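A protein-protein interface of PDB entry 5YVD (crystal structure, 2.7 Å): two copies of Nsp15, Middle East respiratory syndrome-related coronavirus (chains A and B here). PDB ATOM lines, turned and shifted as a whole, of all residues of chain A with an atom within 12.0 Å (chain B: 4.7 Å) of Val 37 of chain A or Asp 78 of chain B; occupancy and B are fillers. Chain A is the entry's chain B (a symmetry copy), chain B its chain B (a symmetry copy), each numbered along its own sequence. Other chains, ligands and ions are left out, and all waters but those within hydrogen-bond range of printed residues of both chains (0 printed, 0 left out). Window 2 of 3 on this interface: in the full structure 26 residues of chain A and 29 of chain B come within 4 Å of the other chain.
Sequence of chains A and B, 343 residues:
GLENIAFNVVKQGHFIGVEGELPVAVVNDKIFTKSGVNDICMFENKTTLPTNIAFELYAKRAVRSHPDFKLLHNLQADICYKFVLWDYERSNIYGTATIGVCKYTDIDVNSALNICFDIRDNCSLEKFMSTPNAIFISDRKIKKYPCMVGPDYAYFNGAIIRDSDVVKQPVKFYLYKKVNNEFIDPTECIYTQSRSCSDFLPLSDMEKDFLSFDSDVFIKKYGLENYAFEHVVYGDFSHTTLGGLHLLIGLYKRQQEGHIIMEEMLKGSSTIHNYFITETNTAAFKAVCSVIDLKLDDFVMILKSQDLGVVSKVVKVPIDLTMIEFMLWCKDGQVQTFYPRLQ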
ATOM      1  N   LEU A  22      19.199   7.644   8.553  1.00  0.00           N
ATOM      2  CA  LEU A  22      19.973   8.215   9.647  1.00  0.00           C
ATOM      3  C   LEU A  22      20.488   9.578   9.201  1.00  0.00           C
ATOM      4  O   LEU A  22      20.699   9.802   8.005  1.00  0.00           O
ATOM      5  CB  LEU A  22      21.135   7.323  10.039  1.00  0.00           C
ATOM      6  CG  LEU A  22      20.810   6.005  10.755  1.00  0.00           C
ATOM      7  CD1 LEU A  22      22.111   5.277  11.065  1.00  0.00           C
ATOM      8  CD2 LEU A  22      19.985   6.188  12.034  1.00  0.00           C
ATOM      9  N   PRO A  23      20.677  10.504  10.152  1.00  0.00           N
ATOM     10  CA  PRO A  23      21.263  11.789   9.776  1.00  0.00           C
ATOM     11  C   PRO A  23      22.727  11.603   9.446  1.00  0.00           C
ATOM     12  O   PRO A  23      23.389  10.770  10.053  1.00  0.00           O
ATOM     13  CB  PRO A  23      21.089  12.651  11.019  1.00  0.00           C
ATOM     14  CG  PRO A  23      20.884  11.691  12.147  1.00  0.00           C
ATOM     15  CD  PRO A  23      20.547  10.331  11.603  1.00  0.00           C
ATOM     16  N   ALA A  25      26.358  13.759   7.898  1.00  0.00           N
ATOM     17  CA  ALA A  25      27.171  14.847   7.335  1.00  0.00           C
ATOM     18  C   ALA A  25      28.134  14.304   6.282  1.00  0.00           C
ATOM     19  O   ALA A  25      28.751  13.263   6.508  1.00  0.00           O
ATOM     20  CB  ALA A  25      27.938  15.549   8.443  1.00  0.00           C
ATOM     21  N   PHE A  32      30.130  11.214   8.136  1.00  0.00           N
ATOM     22  CA  PHE A  32      29.793  11.064   9.555  1.00  0.00           C
ATOM     23  C   PHE A  32      28.298  10.819   9.733  1.00  0.00           C
ATOM     24  O   PHE A  32      27.499  11.245   8.901  1.00  0.00           O
ATOM     25  CB  PHE A  32      30.198  12.311  10.351  1.00  0.00           C
ATOM     26  CG  PHE A  32      31.686  12.562  10.414  1.00  0.00           C
ATOM     27  CD1 PHE A  32      32.421  12.172  11.532  1.00  0.00           C
ATOM     28  CD2 PHE A  32      32.337  13.208   9.377  1.00  0.00           C
ATOM     29  CE1 PHE A  32      33.780  12.397  11.606  1.00  0.00           C
ATOM     30  CE2 PHE A  32      33.689  13.448   9.444  1.00  0.00           C
ATOM     31  CZ  PHE A  32      34.412  13.042  10.562  1.00  0.00           C
ATOM     32  N   THR A  33      27.927  10.123  10.803  1.00  0.00           N
ATOM     33  CA  THR A  33      26.518  10.045  11.199  1.00  0.00           C
ATOM     34  C   THR A  33      26.316  10.472  12.663  1.00  0.00           C
ATOM     35  O   THR A  33      27.203  10.270  13.505  1.00  0.00           O
ATOM     36  CB  THR A  33      25.940   8.646  10.986  1.00  0.00           C
ATOM     37  OG1 THR A  33      24.525   8.710  11.079  1.00  0.00           O
ATOM     38  CG2 THR A  33      26.481   7.626  12.033  1.00  0.00           C
ATOM     39  N   LYS A  34      25.160  11.075  12.955  1.00  0.00           N
ATOM     40  CA  LYS A  34      24.840  11.479  14.326  1.00  0.00           C
ATOM     41  C   LYS A  34      24.285  10.282  15.035  1.00  0.00           C
ATOM     42  O   LYS A  34      23.185   9.873  14.740  1.00  0.00           O
ATOM     43  CB  LYS A  34      23.819  12.631  14.400  1.00  0.00           C
ATOM     44  CG  LYS A  34      24.431  13.981  14.758  1.00  0.00           C
ATOM     45  CD  LYS A  34      23.705  14.696  15.905  1.00  0.00           C
ATOM     46  CE  LYS A  34      24.275  16.099  16.189  1.00  0.00           C
ATOM     47  NZ  LYS A  34      25.680  16.374  15.727  1.00  0.00           N
ATOM     48  N   SER A  35      25.067   9.716  15.945  1.00  0.00           N
ATOM     49  CA  SER A  35      24.614   8.637  16.804  1.00  0.00           C
ATOM     50  C   SER A  35      24.586   9.202  18.207  1.00  0.00           C
ATOM     51  O   SER A  35      25.622   9.604  18.735  1.00  0.00           O
ATOM     52  CB  SER A  35      25.574   7.446  16.722  1.00  0.00           C
ATOM     53  OG  SER A  35      25.175   6.402  17.586  1.00  0.00           O
ATOM     54  N   GLY A  36      23.399   9.229  18.810  1.00  0.00           N
ATOM     55  CA  GLY A  36      23.227   9.854  20.108  1.00  0.00           C
ATOM     56  C   GLY A  36      23.716  11.277  20.006  1.00  0.00           C
ATOM     57  O   GLY A  36      23.238  12.035  19.158  1.00  0.00           O
ATOM     58  N   VAL A  37      24.695  11.629  20.837  1.00  0.00           N
ATOM     59  CA  VAL A  37      25.193  13.006  20.905  1.00  0.00           C
ATOM     60  C   VAL A  37      26.533  13.176  20.162  1.00  0.00           C
ATOM     61  O   VAL A  37      27.088  14.274  20.077  1.00  0.00           O
ATOM     62  CB  VAL A  37      25.299  13.453  22.376  1.00  0.00           C
ATOM     63  CG1 VAL A  37      26.428  12.719  23.098  1.00  0.00           C
ATOM     64  CG2 VAL A  37      25.474  14.964  22.464  1.00  0.00           C
ATOM     65  N   ASN A  38      27.028  12.081  19.600  1.00  0.00           N
ATOM     66  CA  ASN A  38      28.294  12.052  18.875  1.00  0.00           C
ATOM     67  C   ASN A  38      28.161  11.943  17.347  1.00  0.00           C
ATOM     68  O   ASN A  38      27.256  11.300  16.851  1.00  0.00           O
ATOM     69  CB  ASN A  38      29.118  10.859  19.367  1.00  0.00           C
ATOM     70  CG  ASN A  38      29.697  11.082  20.741  1.00  0.00           C
ATOM     71  OD1 ASN A  38      30.364  12.095  21.002  1.00  0.00           O
ATOM     72  ND2 ASN A  38      29.451  10.137  21.631  1.00  0.00           N
ATOM     73  N   ASP A  39      29.092  12.565  16.623  1.00  0.00           N
ATOM     74  CA  ASP A  39      29.266  12.367  15.190  1.00  0.00           C
ATOM     75  C   ASP A  39      30.263  11.242  14.939  1.00  0.00           C
ATOM     76  O   ASP A  39      31.405  11.335  15.336  1.00  0.00           O
ATOM     77  CB  ASP A  39      29.832  13.618  14.531  1.00  0.00           C
ATOM     78  CG  ASP A  39      28.954  14.823  14.688  1.00  0.00           C
ATOM     79  OD1 ASP A  39      27.760  14.754  14.346  1.00  0.00           O
ATOM     80  OD2 ASP A  39      29.496  15.857  15.140  1.00  0.00           O
ATOM     81  N   ILE A  40      29.846  10.190  14.245  1.00  0.00           N
ATOM     82  CA  ILE A  40      30.692   9.006  14.088  1.00  0.00           C
ATOM     83  C   ILE A  40      30.996   8.717  12.644  1.00  0.00           C
ATOM     84  O   ILE A  40      30.091   8.629  11.808  1.00  0.00           O
ATOM     85  CB  ILE A  40      30.060   7.768  14.750  1.00  0.00           C
ATOM     86  CG1 ILE A  40      29.995   7.999  16.261  1.00  0.00           C
ATOM     87  CG2 ILE A  40      30.865   6.520  14.408  1.00  0.00           C
ATOM     88  CD1 ILE A  40      29.232   6.939  17.009  1.00  0.00           C
ATOM     89  N   CYS A  41      32.285   8.548  12.383  1.00  0.00           N
ATOM     90  CA  CYS A  41      32.824   8.409  11.037  1.00  0.00           C
ATOM     91  C   CYS A  41      32.506   7.025  10.485  1.00  0.00           C
ATOM     92  O   CYS A  41      32.960   6.023  11.021  1.00  0.00           O
ATOM     93  CB  CYS A  41      34.345   8.643  11.061  1.00  0.00           C
ATOM     94  SG  CYS A  41      35.071   8.832   9.422  1.00  0.00           S
ATOM     95  N   GLN B  76      23.081   9.090  29.145  1.00  0.00           N
ATOM     96  CA  GLN B  76      22.599  10.161  28.269  1.00  0.00           C
ATOM     97  C   GLN B  76      23.243  11.497  28.579  1.00  0.00           C
ATOM     98  O   GLN B  76      22.634  12.558  28.365  1.00  0.00           O
ATOM     99  CB  GLN B  76      21.073  10.277  28.290  1.00  0.00           C
ATOM    100  CG  GLN B  76      20.373   9.060  27.706  1.00  0.00           C
ATOM    101  CD  GLN B  76      19.068   8.747  28.418  1.00  0.00           C
ATOM    102  OE1 GLN B  76      19.039   8.632  29.651  1.00  0.00           O
ATOM    103  NE2 GLN B  76      17.979   8.601  27.651  1.00  0.00           N
ATOM    104  N   ALA B  77      24.480  11.446  29.065  1.00  0.00           N
ATOM    105  CA  ALA B  77      25.293  12.652  29.190  1.00  0.00           C
ATOM    106  C   ALA B  77      25.382  13.347  27.845  1.00  0.00           C
ATOM    107  O   ALA B  77      25.707  12.702  26.859  1.00  0.00           O
ATOM    108  CB  ALA B  77      26.681  12.302  29.665  1.00  0.00           C
ATOM    109  N   ASP B  78      25.082  14.649  27.821  1.00  0.00           N
ATOM    110  CA  ASP B  78      25.044  15.460  26.590  1.00  0.00           C
ATOM    111  C   ASP B  78      26.328  16.249  26.387  1.00  0.00           C
ATOM    112  O   ASP B  78      26.785  16.424  25.258  1.00  0.00           O
ATOM    113  CB  ASP B  78      23.851  16.441  26.615  1.00  0.00           C
ATOM    114  CG  ASP B  78      22.487  15.734  26.502  1.00  0.00           C
ATOM    115  OD1 ASP B  78      22.341  14.824  25.658  1.00  0.00           O
ATOM    116  OD2 ASP B  78      21.555  16.077  27.263  1.00  0.00           O
ATOM    117  N   ILE B  79      26.912  16.720  27.486  1.00  0.00           N
ATOM    118  CA  ILE B  79      27.983  17.711  27.454  1.00  0.00           C
ATOM    119  C   ILE B  79      28.657  17.683  28.823  1.00  0.00           C
ATOM    120  O   ILE B  79      28.040  17.191  29.781  1.00  0.00           O
ATOM    121  CB  ILE B  79      27.391  19.095  27.167  1.00  0.00           C
ATOM    122  CG1 ILE B  79      28.488  20.140  26.923  1.00  0.00           C
ATOM    123  CG2 ILE B  79      26.476  19.526  28.296  1.00  0.00           C
ATOM    124  CD1 ILE B  79      27.949  21.475  26.443  1.00  0.00           C
ATOM    125  N   TYR B  94      34.013  13.550  23.208  1.00  0.00           N
ATOM    126  CA  TYR B  94      32.659  13.084  23.554  1.00  0.00           C
ATOM    127  C   TYR B  94      31.707  14.280  23.382  1.00  0.00           C
ATOM    128  O   TYR B  94      31.815  15.265  24.111  1.00  0.00           O
ATOM    129  CB  TYR B  94      32.554  12.549  24.986  1.00  0.00           C
ATOM    130  CG  TYR B  94      31.157  12.059  25.321  1.00  0.00           C
ATOM    131  CD1 TYR B  94      30.213  12.885  25.933  1.00  0.00           C
ATOM    132  CD2 TYR B  94      30.769  10.781  24.988  1.00  0.00           C
ATOM    133  CE1 TYR B  94      28.928  12.430  26.215  1.00  0.00           C
ATOM    134  CE2 TYR B  94      29.492  10.315  25.255  1.00  0.00           C
ATOM    135  CZ  TYR B  94      28.577  11.136  25.871  1.00  0.00           C
ATOM    136  OH  TYR B  94      27.333  10.618  26.119  1.00  0.00           O
ATOM    137  N   GLY B  95      30.790  14.195  22.420  1.00  0.00           N
ATOM    138  CA  GLY B  95      29.856  15.278  22.131  1.00  0.00           C
ATOM    139  C   GLY B  95      30.374  16.236  21.080  1.00  0.00           C
ATOM    140  O   GLY B  95      31.354  15.937  20.401  1.00  0.00           O
ATOM    141  N   THR B  96      29.708  17.378  20.932  1.00  0.00           N
ATOM    142  CA  THR B  96      30.110  18.387  19.938  1.00  0.00           C
ATOM    143  C   THR B  96      30.194  19.805  20.463  1.00  0.00           C
ATOM    144  O   THR B  96      30.895  20.636  19.872  1.00  0.00           O
ATOM    145  CB  THR B  96      29.130  18.434  18.778  1.00  0.00           C
ATOM    146  OG1 THR B  96      27.816  18.602  19.304  1.00  0.00           O
ATOM    147  CG2 THR B  96      29.200  17.122  17.976  1.00  0.00           C
ATOM    148  N   LEU B 113      19.820  19.944  28.963  1.00  0.00           N
ATOM    149  CA  LEU B 113      20.742  18.883  28.702  1.00  0.00           C
ATOM    150  C   LEU B 113      21.216  18.221  29.955  1.00  0.00           C
ATOM    151  O   LEU B 113      21.207  18.787  31.002  1.00  0.00           O
ATOM    152  CB  LEU B 113      21.941  19.458  28.014  1.00  0.00           C
ATOM    153  CG  LEU B 113      21.635  20.746  27.307  1.00  0.00           C
ATOM    154  CD1 LEU B 113      22.321  21.876  28.044  1.00  0.00           C
ATOM    155  CD2 LEU B 113      22.158  20.611  25.898  1.00  0.00           C
ATOM    156  N   ASN B 114      21.665  17.003  29.825  1.00  0.00           N
ATOM    157  CA  ASN B 114      22.210  16.306  30.970  1.00  0.00           C
ATOM    158  C   ASN B 114      23.656  16.687  31.054  1.00  0.00           C
ATOM    159  O   ASN B 114      24.492  16.210  30.292  1.00  0.00           O
ATOM    160  CB  ASN B 114      22.050  14.787  30.863  1.00  0.00           C
ATOM    161  CG  ASN B 114      20.630  14.328  31.142  1.00  0.00           C
ATOM    162  OD1 ASN B 114      20.159  14.344  32.291  1.00  0.00           O
ATOM    163  ND2 ASN B 114      19.944  13.898  30.095  1.00  0.00           N
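OD1 of Asp 39 of chain A lies within salt-bridge range of NZ of Lys 34 of chain A, 3.0 Å away.
O of Ala 77 of chain B lies within hydrogen-bond range of OH of Tyr 94 of chain B, at 2.7 Å.
OD2 of Asp 78 of chain B lies within hydrogen-bond range of N of Asn 114 of chain B.
Leu 22 of chain A touches none of the printed residues of chain B.
Pro 23 of chain A touches none of the printed residues of chain B.
Of the printed residues of chain B, Asn 38 of chain A touches Tyr 94 (3.5 Å) and Gly 95 (2.6 Å).
Of the printed residues of chain B, Asp 39 of chain A touches Thr 96.
Ala 77 of chain B touches just one residue of chain A: Val 37.
Of chain A, only Val 37 comes within 4 Å of Asp 78 of chain B.
No residue of chain A comes within 4 Å of Ile 79 of chain B.
Of chain A, only Val 37 (3.8 Å) and Asn 38 (3.5 Å) come within 4 Å of Tyr 94 of chain B.
Gly 95 of chain B touches just these residues of chain A: Val 37 and Asn 38.
No residue of chain A comes within 4 Å of Leu 113 of chain B.
The nearest printed residue of chain B that does not touch Asp 39 of chain A is Gly 95 of chain B (5.5 Å).
Hydrophobic or aromatic side chains of chain A within 4 Å of the printed part of chain B: Val 37.
Hydrophobic or aromatic side chains of chain B within 4 Å of the printed part of chain A: Tyr 94.
Among the printed residues, 7 pairs touch across the chains.
Among the printed residues, no Asp or Glu carboxylate lies within 4 Å of a Lys or Arg side-chain nitrogen of the other chain.
The side-chain amide oxygen (OD1) of Asn 38 of chain A sits at hydrogen-bond distance from the backbone NH (N) of Gly 95 of chain B.
No position is printed for both chains.
Of the 7 pairs that touch across the chains among the printed residues, none has its exchanged pair printed and touching as well.
Among the printed residues, pairs that only touch across the chains: Asp 39 of chain A with Thr 96 of chain B, Val 37 of chain A with Asp 78 of chain B, Asn 38 of chain A with Tyr 94 of chain B, Val 37 of chain A with Gly 95 of chain B, Val 37 of chain A with Tyr 94 of chain B and Val 37 of chain A with Ala 77 of chain B.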
